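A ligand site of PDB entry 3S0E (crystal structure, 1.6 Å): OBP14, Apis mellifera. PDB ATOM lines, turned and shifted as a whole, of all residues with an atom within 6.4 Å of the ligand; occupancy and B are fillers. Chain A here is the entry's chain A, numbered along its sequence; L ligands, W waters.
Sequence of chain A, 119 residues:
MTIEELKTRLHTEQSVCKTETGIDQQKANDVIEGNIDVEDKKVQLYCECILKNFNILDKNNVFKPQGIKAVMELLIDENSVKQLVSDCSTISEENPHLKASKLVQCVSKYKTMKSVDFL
O of Leu 51 is in hydrogen-bond range of N of Ile 56 (2.8 Å).
The backbone carbonyl oxygen (O) of Val 104 lies within hydrogen-bond range of the side-chain hydroxyl (OG) of Ser 108.
The side-chain hydroxyl (OG) of Ser 115 sits at hydrogen-bond distance from the backbone carbonyl oxygen (O) of Thr 112 (2.7 Å).
The backbone NH (N) of Met 113 is in hydrogen-bond range of the backbone carbonyl oxygen (O) of Ile 32 (3.3 Å).
The backbone carbonyl oxygen (O) of Thr 112 lies close to an oxygen (O2) of the ligand, 3.5 Å away.
CG2 of Ile 50 touches C7 of the ligand, at 3.9 Å.
Phe 54 touches the ligand (CG to C8, 3.95 Å).
Ile 56 touches the ligand.
Ile 68 touches the ligand.
CG1 of Val 71 touches C9 of the ligand (3.6 Å).
SD of Met 72 touches C10 of the ligand, at 3.9 Å.
CD1 of Leu 75 touches C10 of the ligand (3.4 Å).
Val 104 touches the ligand.
Val 107 touches the ligand (CG1 to C5, 3.5 Å).
Met 113 touches the ligand (N to O2, 3.5 Å).
13 residues have an atom within 4 Å of the ligand: Ile 50, Phe 54, Ile 56, Ile 68, Val 71, Met 72, Leu 75, Val 104, Val 107, Ser 108, Lys 111, Thr 112 and Met 113.
The nearest printed residue that does not touch the ligand is Val 116 (4.1 Å).
Water W1 lies within hydrogen-bond range of N of Met 113 (2.9 Å), O of Val 31 (3.0 Å), OG of Ser 108 (3.1 Å), O1 of the ligand (3.1 Å) and O of Ile 32 (3.3 Å).
An oxygen (O1) of the ligand sits at hydrogen-bond distance from the backbone carbonyl oxygen (O) of Lys 111 (2.6 Å).
O1 of the ligand lies within hydrogen-bond range of OG of Ser 108, 3.2 Å away.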
ATOM      1  N   LEU A   6       2.757 -13.711  -0.827  1.00  0.00           N
ATOM      2  CA  LEU A   6       4.109 -13.344  -0.407  1.00  0.00           C
ATOM      3  C   LEU A   6       4.111 -12.939   1.070  1.00  0.00           C
ATOM      4  O   LEU A   6       5.022 -13.330   1.806  1.00  0.00           O
ATOM      5  CB  LEU A   6       4.710 -12.237  -1.293  1.00  0.00           C
ATOM      6  CG  LEU A   6       6.113 -11.706  -0.895  1.00  0.00           C
ATOM      7  CD1 LEU A   6       7.173 -12.805  -0.884  1.00  0.00           C
ATOM      8  CD2 LEU A   6       6.530 -10.546  -1.773  1.00  0.00           C
ATOM      9  N   LEU A  10       6.360 -14.823   3.705  1.00  0.00           N
ATOM     10  CA  LEU A  10       7.359 -14.116   4.533  1.00  0.00           C
ATOM     11  C   LEU A  10       7.113 -14.377   6.003  1.00  0.00           C
ATOM     12  O   LEU A  10       8.063 -14.690   6.713  1.00  0.00           O
ATOM     13  CB  LEU A  10       7.343 -12.611   4.251  1.00  0.00           C
ATOM     14  CG  LEU A  10       8.035 -12.163   2.973  1.00  0.00           C
ATOM     15  CD1 LEU A  10       7.578 -10.767   2.585  1.00  0.00           C
ATOM     16  CD2 LEU A  10       9.559 -12.185   3.124  1.00  0.00           C
ATOM     17  N   VAL A  31      15.654  -6.812  11.639  1.00  0.00           N
ATOM     18  CA  VAL A  31      15.972  -7.326  10.299  1.00  0.00           C
ATOM     19  C   VAL A  31      14.776  -7.129   9.362  1.00  0.00           C
ATOM     20  O   VAL A  31      14.942  -6.628   8.240  1.00  0.00           O
ATOM     21  CB  VAL A  31      16.398  -8.819  10.370  1.00  0.00           C
ATOM     22  CG1 VAL A  31      16.503  -9.442   8.976  1.00  0.00           C
ATOM     23  CG2 VAL A  31      17.719  -8.969  11.142  1.00  0.00           C
ATOM     24  N   ILE A  32      13.579  -7.443   9.840  1.00  0.00           N
ATOM     25  CA  ILE A  32      12.368  -7.323   9.033  1.00  0.00           C
ATOM     26  C   ILE A  32      12.125  -5.851   8.658  1.00  0.00           C
ATOM     27  O   ILE A  32      11.628  -5.589   7.566  1.00  0.00           O
ATOM     28  CB  ILE A  32      11.173  -7.967   9.791  1.00  0.00           C
ATOM     29  CG1 ILE A  32      11.383  -9.491   9.939  1.00  0.00           C
ATOM     30  CG2 ILE A  32       9.816  -7.655   9.132  1.00  0.00           C
ATOM     31  CD1 ILE A  32      10.430 -10.170  10.981  1.00  0.00           C
ATOM     32  N   GLY A  34      14.453  -3.700   8.094  1.00  0.00           N
ATOM     33  CA  GLY A  34      15.577  -3.247   7.291  1.00  0.00           C
ATOM     34  C   GLY A  34      16.723  -2.636   8.056  1.00  0.00           C
ATOM     35  O   GLY A  34      17.578  -1.992   7.447  1.00  0.00           O
ATOM     36  N   ILE A  36      19.741  -3.864   9.700  1.00  0.00           N
ATOM     37  CA  ILE A  36      20.537  -5.074   9.794  1.00  0.00           C
ATOM     38  C   ILE A  36      21.885  -4.887  10.467  1.00  0.00           C
ATOM     39  O   ILE A  36      22.747  -4.164   9.958  1.00  0.00           O
ATOM     40  CB  ILE A  36      20.583  -5.821   8.419  1.00  0.00           C
ATOM     41  CG1 ILE A  36      19.149  -6.257   7.995  1.00  0.00           C
ATOM     42  CG2 ILE A  36      21.489  -7.072   8.465  1.00  0.00           C
ATOM     43  CD1 ILE A  36      18.588  -5.495   6.939  1.00  0.00           C
ATOM     44  N   ILE A  50      16.594 -17.222   5.794  1.00  0.00           N
ATOM     45  CA  ILE A  50      15.546 -16.620   4.965  1.00  0.00           C
ATOM     46  C   ILE A  50      15.944 -16.654   3.492  1.00  0.00           C
ATOM     47  O   ILE A  50      15.149 -17.054   2.629  1.00  0.00           O
ATOM     48  CB  ILE A  50      15.220 -15.186   5.444  1.00  0.00           C
ATOM     49  CG1 ILE A  50      14.496 -15.246   6.821  1.00  0.00           C
ATOM     50  CG2 ILE A  50      14.363 -14.423   4.409  1.00  0.00           C
ATOM     51  CD1 ILE A  50      14.296 -13.940   7.466  1.00  0.00           C
ATOM     52  N   LEU A  51      17.182 -16.230   3.178  1.00  0.00           N
ATOM     53  CA  LEU A  51      17.600 -16.236   1.771  1.00  0.00           C
ATOM     54  C   LEU A  51      17.642 -17.615   1.141  1.00  0.00           C
ATOM     55  O   LEU A  51      17.215 -17.781  -0.002  1.00  0.00           O
ATOM     56  CB  LEU A  51      18.929 -15.501   1.552  1.00  0.00           C
ATOM     57  CG  LEU A  51      18.966 -14.018   1.939  1.00  0.00           C
ATOM     58  CD1 LEU A  51      20.390 -13.485   1.783  1.00  0.00           C
ATOM     59  CD2 LEU A  51      17.993 -13.186   1.087  1.00  0.00           C
ATOM     60  N   PHE A  54      14.138 -18.925   0.322  1.00  0.00           N
ATOM     61  CA  PHE A  54      13.555 -18.256  -0.845  1.00  0.00           C
ATOM     62  C   PHE A  54      14.350 -18.543  -2.115  1.00  0.00           C
ATOM     63  O   PHE A  54      14.067 -17.958  -3.159  1.00  0.00           O
ATOM     64  CB  PHE A  54      13.454 -16.749  -0.605  1.00  0.00           C
ATOM     65  CG  PHE A  54      12.194 -16.335   0.104  1.00  0.00           C
ATOM     66  CD1 PHE A  54      11.010 -16.163  -0.603  1.00  0.00           C
ATOM     67  CD2 PHE A  54      12.187 -16.082   1.474  1.00  0.00           C
ATOM     68  CE1 PHE A  54       9.839 -15.745   0.036  1.00  0.00           C
ATOM     69  CE2 PHE A  54      11.028 -15.652   2.110  1.00  0.00           C
ATOM     70  CZ  PHE A  54       9.866 -15.486   1.393  1.00  0.00           C
ATOM     71  N   ILE A  56      17.420 -17.752  -2.837  1.00  0.00           N
ATOM     72  CA  ILE A  56      18.222 -16.561  -3.186  1.00  0.00           C
ATOM     73  C   ILE A  56      19.697 -16.857  -2.997  1.00  0.00           C
ATOM     74  O   ILE A  56      20.550 -16.214  -3.620  1.00  0.00           O
ATOM     75  CB  ILE A  56      17.702 -15.307  -2.456  1.00  0.00           C
ATOM     76  CG1 ILE A  56      16.271 -15.000  -2.946  1.00  0.00           C
ATOM     77  CG2 ILE A  56      18.632 -14.081  -2.646  1.00  0.00           C
ATOM     78  CD1 ILE A  56      15.518 -14.215  -2.069  1.00  0.00           C
ATOM     79  N   GLY A  67      16.071 -15.934  -8.047  1.00  0.00           N
ATOM     80  CA  GLY A  67      15.356 -16.050  -6.781  1.00  0.00           C
ATOM     81  C   GLY A  67      14.903 -14.692  -6.277  1.00  0.00           C
ATOM     82  O   GLY A  67      13.750 -14.540  -5.861  1.00  0.00           O
ATOM     83  N   ILE A  68      15.813 -13.686  -6.316  1.00  0.00           N
ATOM     84  CA  ILE A  68      15.496 -12.325  -5.875  1.00  0.00           C
ATOM     85  C   ILE A  68      14.512 -11.635  -6.836  1.00  0.00           C
ATOM     86  O   ILE A  68      13.650 -10.897  -6.377  1.00  0.00           O
ATOM     87  CB  ILE A  68      16.761 -11.479  -5.535  1.00  0.00           C
ATOM     88  CG1 ILE A  68      16.419 -10.241  -4.678  1.00  0.00           C
ATOM     89  CG2 ILE A  68      17.528 -11.066  -6.799  1.00  0.00           C
ATOM     90  CD1 ILE A  68      15.940 -10.495  -3.290  1.00  0.00           C
ATOM     91  N   VAL A  71      10.814 -12.612  -6.166  1.00  0.00           N
ATOM     92  CA  VAL A  71      10.233 -11.899  -5.035  1.00  0.00           C
ATOM     93  C   VAL A  71      10.076 -10.405  -5.345  1.00  0.00           C
ATOM     94  O   VAL A  71       8.970  -9.870  -5.206  1.00  0.00           O
ATOM     95  CB  VAL A  71      11.075 -12.118  -3.737  1.00  0.00           C
ATOM     96  CG1 VAL A  71      10.583 -11.253  -2.589  1.00  0.00           C
ATOM     97  CG2 VAL A  71      11.084 -13.597  -3.335  1.00  0.00           C
ATOM     98  N   MET A  72      11.170  -9.730  -5.740  1.00  0.00           N
ATOM     99  CA  MET A  72      11.170  -8.278  -5.940  1.00  0.00           C
ATOM    100  C   MET A  72      10.326  -7.733  -7.072  1.00  0.00           C
ATOM    101  O   MET A  72       9.855  -6.597  -6.962  1.00  0.00           O
ATOM    102  CB  MET A  72      12.593  -7.695  -5.943  1.00  0.00           C
ATOM    103  CG  MET A  72      13.407  -8.047  -4.716  1.00  0.00           C
ATOM    104  SD  MET A  72      12.680  -7.583  -3.119  1.00  0.00           S
ATOM    105  CE  MET A  72      12.890  -5.854  -3.166  1.00  0.00           C
ATOM    106  N   LEU A  75       7.066  -6.312  -5.974  1.00  0.00           N
ATOM    107  CA  LEU A  75       7.177  -5.162  -5.081  1.00  0.00           C
ATOM    108  C   LEU A  75       7.707  -3.858  -5.666  1.00  0.00           C
ATOM    109  O   LEU A  75       7.351  -2.797  -5.157  1.00  0.00           O
ATOM    110  CB  LEU A  75       8.058  -5.542  -3.882  1.00  0.00           C
ATOM    111  CG  LEU A  75       7.724  -6.860  -3.180  1.00  0.00           C
ATOM    112  CD1 LEU A  75       8.749  -7.157  -2.117  1.00  0.00           C
ATOM    113  CD2 LEU A  75       6.327  -6.828  -2.568  1.00  0.00           C
ATOM    114  N   LEU A 103      23.830  -9.244   2.194  1.00  0.00           N
ATOM    115  CA  LEU A 103      22.841  -9.360   1.119  1.00  0.00           C
ATOM    116  C   LEU A 103      21.464  -8.875   1.552  1.00  0.00           C
ATOM    117  O   LEU A 103      20.809  -8.135   0.798  1.00  0.00           O
ATOM    118  CB  LEU A 103      22.772 -10.778   0.566  1.00  0.00           C
ATOM    119  CG  LEU A 103      23.891 -11.134  -0.415  1.00  0.00           C
ATOM    120  CD1 LEU A 103      24.025 -12.619  -0.554  1.00  0.00           C
ATOM    121  CD2 LEU A 103      23.665 -10.474  -1.782  1.00  0.00           C
ATOM    122  N   VAL A 104      20.995  -9.260   2.750  1.00  0.00           N
ATOM    123  CA  VAL A 104      19.706  -8.793   3.258  1.00  0.00           C
ATOM    124  C   VAL A 104      19.762  -7.277   3.438  1.00  0.00           C
ATOM    125  O   VAL A 104      18.805  -6.596   3.091  1.00  0.00           O
ATOM    126  CB  VAL A 104      19.290  -9.551   4.545  1.00  0.00           C
ATOM    127  CG1 VAL A 104      18.098  -8.879   5.229  1.00  0.00           C
ATOM    128  CG2 VAL A 104      18.967 -11.008   4.226  1.00  0.00           C
ATOM    129  N   GLN A 105      20.881  -6.738   3.941  1.00  0.00           N
ATOM    130  CA  GLN A 105      21.051  -5.302   4.098  1.00  0.00           C
ATOM    131  C   GLN A 105      20.948  -4.606   2.725  1.00  0.00           C
ATOM    132  O   GLN A 105      20.285  -3.564   2.612  1.00  0.00           O
ATOM    133  CB  GLN A 105      22.394  -5.013   4.778  1.00  0.00           C
ATOM    134  CG  GLN A 105      22.667  -3.511   4.979  1.00  0.00           C
ATOM    135  CD  GLN A 105      24.020  -3.285   5.598  1.00  0.00           C
ATOM    136  OE1 GLN A 105      25.055  -3.655   5.039  1.00  0.00           O
ATOM    137  NE2 GLN A 105      24.030  -2.682   6.776  1.00  0.00           N
ATOM    138  N   VAL A 107      19.367  -5.778  -0.130  1.00  0.00           N
ATOM    139  CA  VAL A 107      17.980  -5.871  -0.612  1.00  0.00           C
ATOM    140  C   VAL A 107      17.094  -4.845   0.140  1.00  0.00           C
ATOM    141  O   VAL A 107      16.222  -4.223  -0.472  1.00  0.00           O
ATOM    142  CB  VAL A 107      17.403  -7.303  -0.482  1.00  0.00           C
ATOM    143  CG1 VAL A 107      15.939  -7.359  -0.943  1.00  0.00           C
ATOM    144  CG2 VAL A 107      18.242  -8.330  -1.257  1.00  0.00           C
ATOM    145  N   SER A 108      17.317  -4.690   1.457  1.00  0.00           N
ATOM    146  CA  SER A 108      16.542  -3.817   2.350  1.00  0.00           C
ATOM    147  C   SER A 108      16.553  -2.343   1.975  1.00  0.00           C
ATOM    148  O   SER A 108      15.621  -1.626   2.331  1.00  0.00           O
ATOM    149  CB  SER A 108      16.959  -4.002   3.813  1.00  0.00           C
ATOM    150  OG  SER A 108      16.630  -5.304   4.247  1.00  0.00           O
ATOM    151  N   LYS A 109      17.580  -1.907   1.224  1.00  0.00           N
ATOM    152  CA  LYS A 109      17.662  -0.528   0.717  1.00  0.00           C
ATOM    153  C   LYS A 109      16.528  -0.261  -0.292  1.00  0.00           C
ATOM    154  O   LYS A 109      16.099   0.889  -0.448  1.00  0.00           O
ATOM    155  CB  LYS A 109      18.976  -0.288  -0.029  1.00  0.00           C
ATOM    156  CG  LYS A 109      20.244  -0.291   0.816  1.00  0.00           C
ATOM    157  CD  LYS A 109      21.440   0.238   0.011  1.00  0.00           C
ATOM    158  CE  LYS A 109      21.800  -0.626  -1.183  1.00  0.00           C
ATOM    159  NZ  LYS A 109      22.847   0.003  -2.025  1.00  0.00           N
ATOM    160  N   LYS A 111      13.459  -2.491  -0.719  1.00  0.00           N
ATOM    161  CA  LYS A 111      12.202  -2.793  -0.012  1.00  0.00           C
ATOM    162  C   LYS A 111      12.557  -3.652   1.183  1.00  0.00           C
ATOM    163  O   LYS A 111      13.348  -4.579   1.052  1.00  0.00           O
ATOM    164  CB  LYS A 111      11.196  -3.596  -0.866  1.00  0.00           C
ATOM    165  CG  LYS A 111      10.381  -2.812  -1.880  1.00  0.00           C
ATOM    166  CD  LYS A 111       9.648  -1.601  -1.309  1.00  0.00           C
ATOM    167  CE  LYS A 111       8.181  -1.828  -1.181  1.00  0.00           C
ATOM    168  NZ  LYS A 111       7.399  -0.939  -2.087  1.00  0.00           N
ATOM    169  N   THR A 112      11.904  -3.384   2.320  1.00  0.00           N
ATOM    170  CA  THR A 112      12.111  -4.191   3.523  1.00  0.00           C
ATOM    171  C   THR A 112      11.073  -5.296   3.547  1.00  0.00           C
ATOM    172  O   THR A 112      10.054  -5.200   2.866  1.00  0.00           O
ATOM    173  CB  THR A 112      11.998  -3.312   4.774  1.00  0.00           C
ATOM    174  OG1 THR A 112      10.651  -2.859   4.904  1.00  0.00           O
ATOM    175  CG2 THR A 112      12.973  -2.126   4.774  1.00  0.00           C
ATOM    176  N   MET A 113      11.316  -6.343   4.358  1.00  0.00           N
ATOM    177  CA  MET A 113      10.305  -7.404   4.516  1.00  0.00           C
ATOM    178  C   MET A 113       9.050  -6.820   5.160  1.00  0.00           C
ATOM    179  O   MET A 113       7.948  -7.175   4.760  1.00  0.00           O
ATOM    180  CB  MET A 113      10.855  -8.540   5.356  1.00  0.00           C
ATOM    181  CG  MET A 113      11.879  -9.332   4.613  1.00  0.00           C
ATOM    182  SD  MET A 113      12.320 -10.857   5.474  1.00  0.00           S
ATOM    183  CE  MET A 113      13.646 -10.275   6.503  1.00  0.00           C
ATOM    184  N   LYS A 114       9.226  -5.878   6.105  1.00  0.00           N
ATOM    185  CA  LYS A 114       8.083  -5.238   6.785  1.00  0.00           C
ATOM    186  C   LYS A 114       7.175  -4.513   5.796  1.00  0.00           C
ATOM    187  O   LYS A 114       5.944  -4.545   5.953  1.00  0.00           O
ATOM    188  CB  LYS A 114       8.578  -4.244   7.831  1.00  0.00           C
ATOM    189  CG  LYS A 114       7.429  -3.687   8.684  1.00  0.00           C
ATOM    190  CD  LYS A 114       7.888  -2.586   9.590  1.00  0.00           C
ATOM    191  CE  LYS A 114       6.926  -2.342  10.723  1.00  0.00           C
ATOM    192  NZ  LYS A 114       7.458  -1.365  11.708  1.00  0.00           N
ATOM    193  N   SER A 115       7.774  -3.876   4.766  1.00  0.00           N
ATOM    194  CA  SER A 115       7.022  -3.087   3.785  1.00  0.00           C
ATOM    195  C   SER A 115       5.893  -3.864   3.104  1.00  0.00           C
ATOM    196  O   SER A 115       4.866  -3.269   2.760  1.00  0.00           O
ATOM    197  CB  SER A 115       7.962  -2.492   2.738  1.00  0.00           C
ATOM    198  OG  SER A 115       8.362  -3.468   1.785  1.00  0.00           O
ATOM    199  N   VAL A 116       6.067  -5.187   2.959  1.00  0.00           N
ATOM    200  CA  VAL A 116       5.078  -6.055   2.309  1.00  0.00           C
ATOM    201  C   VAL A 116       3.745  -6.103   3.084  1.00  0.00           C
ATOM    202  O   VAL A 116       2.683  -6.248   2.474  1.00  0.00           O
ATOM    203  CB  VAL A 116       5.676  -7.462   2.019  1.00  0.00           C
ATOM    204  CG1 VAL A 116       4.728  -8.331   1.213  1.00  0.00           C
ATOM    205  CG2 VAL A 116       7.013  -7.329   1.279  1.00  0.00           C
HETATM  206  C1  LIG L   1      12.850  -9.688   1.208  1.00  0.00           C
HETATM  207  O1  LIG L   1      14.410  -6.586   2.318  1.00  0.00           O
HETATM  208  C2  LIG L   1      13.815 -10.608   1.626  1.00  0.00           C
HETATM  209  O2  LIG L   1      12.141  -7.367   1.083  1.00  0.00           O
HETATM  210  C3  LIG L   1      13.062  -8.330   1.438  1.00  0.00           C
HETATM  211  C4  LIG L   1      14.988 -10.174   2.245  1.00  0.00           C
HETATM  212  C5  LIG L   1      14.213  -7.909   2.090  1.00  0.00           C
HETATM  213  C6  LIG L   1      15.194  -8.817   2.483  1.00  0.00           C
HETATM  214  C7  LIG L   1      13.608 -12.075   1.426  1.00  0.00           C
HETATM  215  C8  LIG L   1      13.290 -12.539   0.050  1.00  0.00           C
HETATM  216  C9  LIG L   1      13.729 -11.824  -1.015  1.00  0.00           C
HETATM  217  C10 LIG L   1      10.993  -7.717   0.402  1.00  0.00           C
HETATM  218  O   HOH W   1      14.034  -6.451   5.428  1.00  0.00           O
